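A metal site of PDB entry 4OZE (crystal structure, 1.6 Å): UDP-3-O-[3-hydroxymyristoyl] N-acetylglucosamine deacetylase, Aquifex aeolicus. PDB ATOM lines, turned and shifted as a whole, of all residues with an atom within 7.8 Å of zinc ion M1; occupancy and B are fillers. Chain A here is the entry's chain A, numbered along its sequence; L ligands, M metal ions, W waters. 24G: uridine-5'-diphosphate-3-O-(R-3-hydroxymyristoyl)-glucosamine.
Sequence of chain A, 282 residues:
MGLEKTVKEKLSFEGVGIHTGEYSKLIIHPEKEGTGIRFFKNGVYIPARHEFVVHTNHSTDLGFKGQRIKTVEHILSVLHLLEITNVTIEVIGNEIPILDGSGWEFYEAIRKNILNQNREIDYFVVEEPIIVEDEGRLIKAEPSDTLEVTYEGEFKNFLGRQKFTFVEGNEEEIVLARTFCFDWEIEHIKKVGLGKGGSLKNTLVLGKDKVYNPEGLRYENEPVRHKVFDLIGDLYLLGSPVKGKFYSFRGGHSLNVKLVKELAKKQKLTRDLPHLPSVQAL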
ATOM      1  N   HIS A  58     -14.852  -4.819  16.262  1.00  0.00           N
ATOM      2  CA  HIS A  58     -13.403  -4.721  16.436  1.00  0.00           C
ATOM      3  C   HIS A  58     -12.688  -6.071  16.269  1.00  0.00           C
ATOM      4  O   HIS A  58     -11.493  -6.152  16.519  1.00  0.00           O
ATOM      5  CB  HIS A  58     -12.996  -4.047  17.773  1.00  0.00           C
ATOM      6  CG  HIS A  58     -13.627  -2.696  17.946  1.00  0.00           C
ATOM      7  ND1 HIS A  58     -13.177  -1.604  17.236  1.00  0.00           N
ATOM      8  CD2 HIS A  58     -14.707  -2.331  18.680  1.00  0.00           C
ATOM      9  CE1 HIS A  58     -13.974  -0.608  17.579  1.00  0.00           C
ATOM     10  NE2 HIS A  58     -14.921  -1.004  18.431  1.00  0.00           N
ATOM     11  N   SER A  59     -13.415  -7.106  15.836  1.00  0.00           N
ATOM     12  CA  SER A  59     -12.897  -8.444  15.572  1.00  0.00           C
ATOM     13  C   SER A  59     -14.033  -9.286  15.065  1.00  0.00           C
ATOM     14  O   SER A  59     -15.176  -8.897  15.196  1.00  0.00           O
ATOM     15  CB  SER A  59     -12.303  -9.087  16.822  1.00  0.00           C
ATOM     16  OG  SER A  59     -13.233  -9.198  17.892  1.00  0.00           O
ATOM     17  N   THR A  71     -11.748 -13.108  17.779  1.00  0.00           N
ATOM     18  CA  THR A  71     -10.661 -12.749  16.866  1.00  0.00           C
ATOM     19  C   THR A  71     -10.225 -13.923  15.984  1.00  0.00           C
ATOM     20  O   THR A  71      -9.047 -14.309  15.993  1.00  0.00           O
ATOM     21  CB  THR A  71      -9.520 -12.107  17.680  1.00  0.00           C
ATOM     22  OG1 THR A  71     -10.113 -11.208  18.666  1.00  0.00           O
ATOM     23  CG2 THR A  71      -8.511 -11.351  16.781  1.00  0.00           C
ATOM     24  N   GLU A  73     -10.309 -13.914  12.652  1.00  0.00           N
ATOM     25  CA  GLU A  73     -10.021 -13.459  11.286  1.00  0.00           C
ATOM     26  C   GLU A  73      -8.655 -13.840  10.726  1.00  0.00           C
ATOM     27  O   GLU A  73      -8.566 -14.136   9.523  1.00  0.00           O
ATOM     28  CB  GLU A  73     -10.234 -11.915  11.143  1.00  0.00           C
ATOM     29  CG  GLU A  73      -9.499 -11.062  12.165  1.00  0.00           C
ATOM     30  CD  GLU A  73     -10.323 -10.620  13.365  1.00  0.00           C
ATOM     31  OE1 GLU A  73     -11.114 -11.451  13.864  1.00  0.00           O
ATOM     32  OE2 GLU A  73     -10.099  -9.504  13.878  1.00  0.00           O
ATOM     33  N   HIS A  74      -7.622 -13.824  11.549  1.00  0.00           N
ATOM     34  CA  HIS A  74      -6.267 -14.078  11.037  1.00  0.00           C
ATOM     35  C   HIS A  74      -5.985 -15.547  10.823  1.00  0.00           C
ATOM     36  O   HIS A  74      -5.448 -15.907   9.761  1.00  0.00           O
ATOM     37  CB  HIS A  74      -5.208 -13.418  11.934  1.00  0.00           C
ATOM     38  CG  HIS A  74      -5.387 -11.933  12.049  1.00  0.00           C
ATOM     39  ND1 HIS A  74      -4.722 -11.194  13.019  1.00  0.00           N
ATOM     40  CD2 HIS A  74      -6.162 -11.072  11.331  1.00  0.00           C
ATOM     41  CE1 HIS A  74      -5.102  -9.934  12.842  1.00  0.00           C
ATOM     42  NE2 HIS A  74      -6.005  -9.819  11.876  1.00  0.00           N
ATOM     43  N   SER A  77      -7.883 -16.468   7.765  1.00  0.00           N
ATOM     44  CA  SER A  77      -7.327 -15.959   6.504  1.00  0.00           C
ATOM     45  C   SER A  77      -6.189 -16.850   6.042  1.00  0.00           C
ATOM     46  O   SER A  77      -6.159 -17.227   4.873  1.00  0.00           O
ATOM     47  CB  SER A  77      -6.819 -14.537   6.660  1.00  0.00           C
ATOM     48  OG  SER A  77      -6.475 -14.053   5.360  1.00  0.00           O
ATOM     49  N   ILE A  98      -2.912 -13.200  19.297  1.00  0.00           N
ATOM     50  CA  ILE A  98      -2.668 -12.191  18.245  1.00  0.00           C
ATOM     51  C   ILE A  98      -1.270 -12.333  17.646  1.00  0.00           C
ATOM     52  O   ILE A  98      -1.051 -11.931  16.482  1.00  0.00           O
ATOM     53  CB  ILE A  98      -2.943 -10.762  18.783  1.00  0.00           C
ATOM     54  CG1 ILE A  98      -2.918  -9.711  17.630  1.00  0.00           C
ATOM     55  CG2 ILE A  98      -1.948 -10.350  19.916  1.00  0.00           C
ATOM     56  CD1 ILE A  98      -4.044  -9.847  16.625  1.00  0.00           C
ATOM     57  N   GLY A 101       0.367  -9.606  15.305  1.00  0.00           N
ATOM     58  CA  GLY A 101      -0.709  -8.861  14.679  1.00  0.00           C
ATOM     59  C   GLY A 101      -0.915  -9.168  13.204  1.00  0.00           C
ATOM     60  O   GLY A 101      -1.797  -8.600  12.584  1.00  0.00           O
ATOM     61  N   SER A 102      -0.097 -10.098  12.659  1.00  0.00           N
ATOM     62  CA  SER A 102      -0.194 -10.517  11.252  1.00  0.00           C
ATOM     63  C   SER A 102      -0.468 -12.041  11.180  1.00  0.00           C
ATOM     64  O   SER A 102      -0.621 -12.691  12.223  1.00  0.00           O
ATOM     65  CB  SER A 102       1.125 -10.206  10.525  1.00  0.00           C
ATOM     66  OG  SER A 102       2.141 -11.138  10.824  1.00  0.00           O
ATOM     67  N   ALA A 177       1.425  -8.327   6.889  1.00  0.00           N
ATOM     68  CA  ALA A 177       0.786  -7.027   7.196  1.00  0.00           C
ATOM     69  C   ALA A 177       0.062  -7.093   8.545  1.00  0.00           C
ATOM     70  O   ALA A 177      -0.782  -7.975   8.753  1.00  0.00           O
ATOM     71  CB  ALA A 177      -0.163  -6.624   6.065  1.00  0.00           C
ATOM     72  N   ARG A 178       0.410  -6.179   9.451  1.00  0.00           N
ATOM     73  CA  ARG A 178      -0.150  -6.196  10.803  1.00  0.00           C
ATOM     74  C   ARG A 178      -1.406  -5.395  11.014  1.00  0.00           C
ATOM     75  O   ARG A 178      -1.670  -4.410  10.306  1.00  0.00           O
ATOM     76  CB  ARG A 178       0.897  -5.675  11.792  1.00  0.00           C
ATOM     77  CG  ARG A 178       2.148  -6.520  11.840  1.00  0.00           C
ATOM     78  CD  ARG A 178       3.200  -5.723  12.551  1.00  0.00           C
ATOM     79  NE  ARG A 178       3.712  -4.684  11.672  1.00  0.00           N
ATOM     80  CZ  ARG A 178       4.587  -3.757  12.032  1.00  0.00           C
ATOM     81  NH1 ARG A 178       5.004  -3.682  13.290  1.00  0.00           N
ATOM     82  NH2 ARG A 178       5.031  -2.873  11.132  1.00  0.00           N
ATOM     83  N   THR A 179      -2.186  -5.799  12.026  1.00  0.00           N
ATOM     84  CA  THR A 179      -3.385  -5.071  12.436  1.00  0.00           C
ATOM     85  C   THR A 179      -2.946  -3.657  12.903  1.00  0.00           C
ATOM     86  O   THR A 179      -1.779  -3.454  13.290  1.00  0.00           O
ATOM     87  CB  THR A 179      -4.146  -5.809  13.533  1.00  0.00           C
ATOM     88  OG1 THR A 179      -5.366  -5.082  13.770  1.00  0.00           O
ATOM     89  CG2 THR A 179      -3.347  -5.923  14.815  1.00  0.00           C
ATOM     90  N   PHE A 180      -3.856  -2.702  12.809  1.00  0.00           N
ATOM     91  CA  PHE A 180      -3.514  -1.323  13.134  1.00  0.00           C
ATOM     92  C   PHE A 180      -4.683  -0.603  13.754  1.00  0.00           C
ATOM     93  O   PHE A 180      -5.828  -0.984  13.562  1.00  0.00           O
ATOM     94  CB  PHE A 180      -3.060  -0.568  11.855  1.00  0.00           C
ATOM     95  CG  PHE A 180      -4.155  -0.435  10.816  1.00  0.00           C
ATOM     96  CD1 PHE A 180      -4.929   0.726  10.734  1.00  0.00           C
ATOM     97  CD2 PHE A 180      -4.443  -1.490   9.942  1.00  0.00           C
ATOM     98  CE1 PHE A 180      -5.944   0.850   9.770  1.00  0.00           C
ATOM     99  CE2 PHE A 180      -5.488  -1.383   9.016  1.00  0.00           C
ATOM    100  CZ  PHE A 180      -6.223  -0.204   8.911  1.00  0.00           C
ATOM    101  N   HIS A 226      -3.312  -5.251   5.211  1.00  0.00           N
ATOM    102  CA  HIS A 226      -3.944  -5.941   6.338  1.00  0.00           C
ATOM    103  C   HIS A 226      -5.461  -6.078   6.139  1.00  0.00           C
ATOM    104  O   HIS A 226      -6.032  -7.123   6.476  1.00  0.00           O
ATOM    105  CB  HIS A 226      -3.679  -5.232   7.672  1.00  0.00           C
ATOM    106  CG  HIS A 226      -4.137  -6.100   8.811  1.00  0.00           C
ATOM    107  ND1 HIS A 226      -3.380  -7.191   9.247  1.00  0.00           N
ATOM    108  CD2 HIS A 226      -5.345  -6.132   9.438  1.00  0.00           C
ATOM    109  CE1 HIS A 226      -4.124  -7.798  10.158  1.00  0.00           C
ATOM    110  NE2 HIS A 226      -5.301  -7.188  10.314  1.00  0.00           N
ATOM    111  N   LYS A 227      -6.106  -5.032   5.625  1.00  0.00           N
ATOM    112  CA  LYS A 227      -7.565  -5.092   5.420  1.00  0.00           C
ATOM    113  C   LYS A 227      -7.918  -6.141   4.364  1.00  0.00           C
ATOM    114  O   LYS A 227      -8.945  -6.837   4.525  1.00  0.00           O
ATOM    115  CB  LYS A 227      -8.121  -3.719   5.020  1.00  0.00           C
ATOM    116  CG  LYS A 227      -8.001  -2.670   6.140  1.00  0.00           C
ATOM    117  CD  LYS A 227      -8.851  -3.013   7.351  1.00  0.00           C
ATOM    118  CE  LYS A 227     -10.161  -2.300   7.307  1.00  0.00           C
ATOM    119  NZ  LYS A 227     -10.899  -2.396   8.607  1.00  0.00           N
ATOM    120  N   PHE A 229      -6.143  -8.920   3.925  1.00  0.00           N
ATOM    121  CA  PHE A 229      -5.927 -10.141   4.701  1.00  0.00           C
ATOM    122  C   PHE A 229      -7.160 -10.446   5.584  1.00  0.00           C
ATOM    123  O   PHE A 229      -7.659 -11.583   5.616  1.00  0.00           O
ATOM    124  CB  PHE A 229      -4.637  -9.955   5.531  1.00  0.00           C
ATOM    125  CG  PHE A 229      -4.290 -11.108   6.425  1.00  0.00           C
ATOM    126  CD1 PHE A 229      -3.785 -12.294   5.898  1.00  0.00           C
ATOM    127  CD2 PHE A 229      -4.467 -11.008   7.807  1.00  0.00           C
ATOM    128  CE1 PHE A 229      -3.471 -13.369   6.738  1.00  0.00           C
ATOM    129  CE2 PHE A 229      -4.104 -12.071   8.645  1.00  0.00           C
ATOM    130  CZ  PHE A 229      -3.610 -13.253   8.110  1.00  0.00           C
ATOM    131  N   ASP A 230      -7.721  -9.405   6.229  1.00  0.00           N
ATOM    132  CA  ASP A 230      -8.928  -9.585   7.048  1.00  0.00           C
ATOM    133  C   ASP A 230     -10.109 -10.055   6.202  1.00  0.00           C
ATOM    134  O   ASP A 230     -10.852 -10.955   6.614  1.00  0.00           O
ATOM    135  CB  ASP A 230      -9.324  -8.262   7.676  1.00  0.00           C
ATOM    136  CG  ASP A 230      -8.545  -7.922   8.942  1.00  0.00           C
ATOM    137  OD1 ASP A 230      -7.920  -8.857   9.538  1.00  0.00           O
ATOM    138  OD2 ASP A 230      -8.546  -6.741   9.336  1.00  0.00           O
ATOM    139  N   LEU A 231     -10.307  -9.424   5.011  1.00  0.00           N
ATOM    140  CA  LEU A 231     -11.453  -9.789   4.170  1.00  0.00           C
ATOM    141  C   LEU A 231     -11.339 -11.247   3.717  1.00  0.00           C
ATOM    142  O   LEU A 231     -12.366 -11.962   3.675  1.00  0.00           O
ATOM    143  CB  LEU A 231     -11.515  -8.836   2.975  1.00  0.00           C
ATOM    144  CG  LEU A 231     -12.611  -9.090   1.910  1.00  0.00           C
ATOM    145  CD1 LEU A 231     -14.002  -9.420   2.507  1.00  0.00           C
ATOM    146  CD2 LEU A 231     -12.717  -7.885   0.996  1.00  0.00           C
ATOM    147  N   HIS A 253     -14.865  -5.744   9.315  1.00  0.00           N
ATOM    148  CA  HIS A 253     -15.488  -7.043   9.629  1.00  0.00           C
ATOM    149  C   HIS A 253     -17.014  -7.043   9.524  1.00  0.00           C
ATOM    150  O   HIS A 253     -17.568  -7.985   8.966  1.00  0.00           O
ATOM    151  CB  HIS A 253     -15.042  -7.562  11.004  1.00  0.00           C
ATOM    152  CG  HIS A 253     -13.565  -7.753  11.133  1.00  0.00           C
ATOM    153  ND1 HIS A 253     -12.865  -8.613  10.290  1.00  0.00           N
ATOM    154  CD2 HIS A 253     -12.697  -7.248  12.051  1.00  0.00           C
ATOM    155  CE1 HIS A 253     -11.596  -8.572  10.701  1.00  0.00           C
ATOM    156  NE2 HIS A 253     -11.459  -7.777  11.761  1.00  0.00           N
HETATM  157  C36 24G L   1     -11.447   2.112   6.716  1.00  0.00           C
HETATM  158  C37 24G L   1     -11.806   2.267   8.001  1.00  0.00           C
HETATM  159  C35 24G L   1     -11.074   3.259   5.938  1.00  0.00           C
HETATM  160  C33 24G L   1     -11.432   4.651   7.949  1.00  0.00           C
HETATM  161  C13 24G L   1      -8.659  -4.039  16.548  1.00  0.00           C
HETATM  162  C3  24G L   1      -9.317  -5.014  13.382  1.00  0.00           C
HETATM  163  C2  24G L   1      -9.050  -3.779  14.226  1.00  0.00           C
HETATM  164  C1  24G L   1      -8.387  -2.654  13.435  1.00  0.00           C
HETATM  165  C26 24G L   1     -13.544   2.946  11.862  1.00  0.00           C
HETATM  166  C27 24G L   1     -13.642   3.161  10.348  1.00  0.00           C
HETATM  167  C25 24G L   1     -12.101   2.458  12.043  1.00  0.00           C
HETATM  168  C6  24G L   1      -9.203  -2.336  12.184  1.00  0.00           C
HETATM  169  C28 24G L   1     -12.235   3.666  10.045  1.00  0.00           C
HETATM  170  C4  24G L   1     -10.126  -4.598  12.040  1.00  0.00           C
HETATM  171  C52 24G L   1       1.826   0.614  25.054  1.00  0.00           C
HETATM  172  C14 24G L   1      -7.583  -4.283  17.555  1.00  0.00           C
HETATM  173  C24 24G L   1     -11.936   0.958  12.176  1.00  0.00           C
HETATM  174  C7  24G L   1      -8.500  -1.343  11.296  1.00  0.00           C
HETATM  175  C51 24G L   1       0.624   1.283  24.458  1.00  0.00           C
HETATM  176  C50 24G L   1       0.131   0.577  23.224  1.00  0.00           C
HETATM  177  C49 24G L   1      -1.156   1.113  22.673  1.00  0.00           C
HETATM  178  C48 24G L   1      -1.877   0.115  21.809  1.00  0.00           C
HETATM  179  C47 24G L   1      -3.048  -0.505  22.475  1.00  0.00           C
HETATM  180  C46 24G L   1      -4.361   0.130  22.089  1.00  0.00           C
HETATM  181  C45 24G L   1      -5.529  -0.764  22.346  1.00  0.00           C
HETATM  182  C44 24G L   1      -5.498  -2.022  21.518  1.00  0.00           C
HETATM  183  C43 24G L   1      -6.137  -1.841  20.214  1.00  0.00           C
HETATM  184  C42 24G L   1      -6.329  -3.126  19.447  1.00  0.00           C
HETATM  185  C40 24G L   1      -7.359  -3.005  18.352  1.00  0.00           C
HETATM  186  N34 24G L   1     -11.099   4.460   6.628  1.00  0.00           N
HETATM  187  N32 24G L   1     -11.814   3.507   8.619  1.00  0.00           N
HETATM  188  N11 24G L   1     -10.054  -6.092  14.111  1.00  0.00           N
HETATM  189  O39 24G L   1     -10.733   3.259   4.755  1.00  0.00           O
HETATM  190  O38 24G L   1     -11.355   5.755   8.466  1.00  0.00           O
HETATM  191  O15 24G L   1      -9.777  -3.673  16.806  1.00  0.00           O
HETATM  192  O18 24G L   1     -12.607  -4.325  10.381  1.00  0.00           O
HETATM  193  O21 24G L   1     -14.498  -0.671  11.509  1.00  0.00           O
HETATM  194  O29 24G L   1     -11.365   2.941  10.883  1.00  0.00           O
HETATM  195  O5  24G L   1      -9.412  -3.540  11.392  1.00  0.00           O
HETATM  196  O9  24G L   1      -8.319  -1.476  14.227  1.00  0.00           O
HETATM  197  O30 24G L   1     -13.779   4.140  12.617  1.00  0.00           O
HETATM  198  O31 24G L   1     -14.646   4.086   9.970  1.00  0.00           O
HETATM  199  O8  24G L   1      -9.342  -0.877  10.239  1.00  0.00           O
HETATM  200  O41 24G L   1      -6.988  -1.979  17.440  1.00  0.00           O
HETATM  201  O17 24G L   1     -13.932  -3.892  12.530  1.00  0.00           O
HETATM  202  O22 24G L   1     -13.302  -1.235   9.324  1.00  0.00           O
HETATM  203  O10 24G L   1      -8.189  -4.186  15.300  1.00  0.00           O
HETATM  204  O12 24G L   1     -11.287  -4.176  12.562  1.00  0.00           O
HETATM  205  O23 24G L   1     -12.264   0.327  10.929  1.00  0.00           O
HETATM  206  O19 24G L   1     -12.450  -2.100  11.517  1.00  0.00           O
HETATM  207  P16 24G L   1     -12.740  -3.661  11.682  1.00  0.00           P
HETATM  208  P20 24G L   1     -13.252  -0.931  10.767  1.00  0.00           P
HETATM  209 ZN    ZN M   1      -6.884  -8.155  11.100  1.00  0.00          ZN
HETATM  210 ZN    ZN M   2      -9.858  -7.736  12.875  1.00  0.00          ZN
HETATM  211  O   HOH W   1      -7.937  -7.519  12.524  1.00  0.00           O
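O10 of the ligand sits at hydrogen-bond distance from OG1 of Thr 179, 3.3 Å away.
The backbone NH of His 253 sits at hydrogen-bond distance from an oxygen (O18) of the ligand (2.9 Å).
The side-chain amino group (NZ) of Lys 227 lies within salt-bridge range of an oxygen (O22) of the ligand, at 2.8 Å.
O9 of the ligand lies within hydrogen-bond range of O of Phe 180 (2.6 Å).
A nitrogen (N11) of the ligand lies close to the backbone carbonyl oxygen (O) of His 58 (2.8 Å).
ND1 of His 226 is in hydrogen-bond range of N of Thr 179 (3.3 Å).
A ring nitrogen (ND1) of His 226 lies close to the backbone carbonyl oxygen of Arg 178 (3.4 Å).
O of Ala 177 sits at hydrogen-bond distance from ND1 of His 226, 2.8 Å away.
Within 4 Å of zinc ion M1: His 74, His 226 and Asp 230.
The nearest printed residue that does not touch zinc ion M1 is Glu 73 (4.1 Å).
Zinc ion M1 is bound by water W1 (1.9 Å), the side-chain carboxylate (OD1) of Asp 230 (2.0 Å), a ring nitrogen (NE2) of His 226 (2.0 Å) and a ring nitrogen (NE2) of His 74 (2.0 Å).
Zinc ion M1 has four donor atoms within binding distance.
Slightly farther from zinc ion M1 lies OD2 of Asp 230 (2.8 Å).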
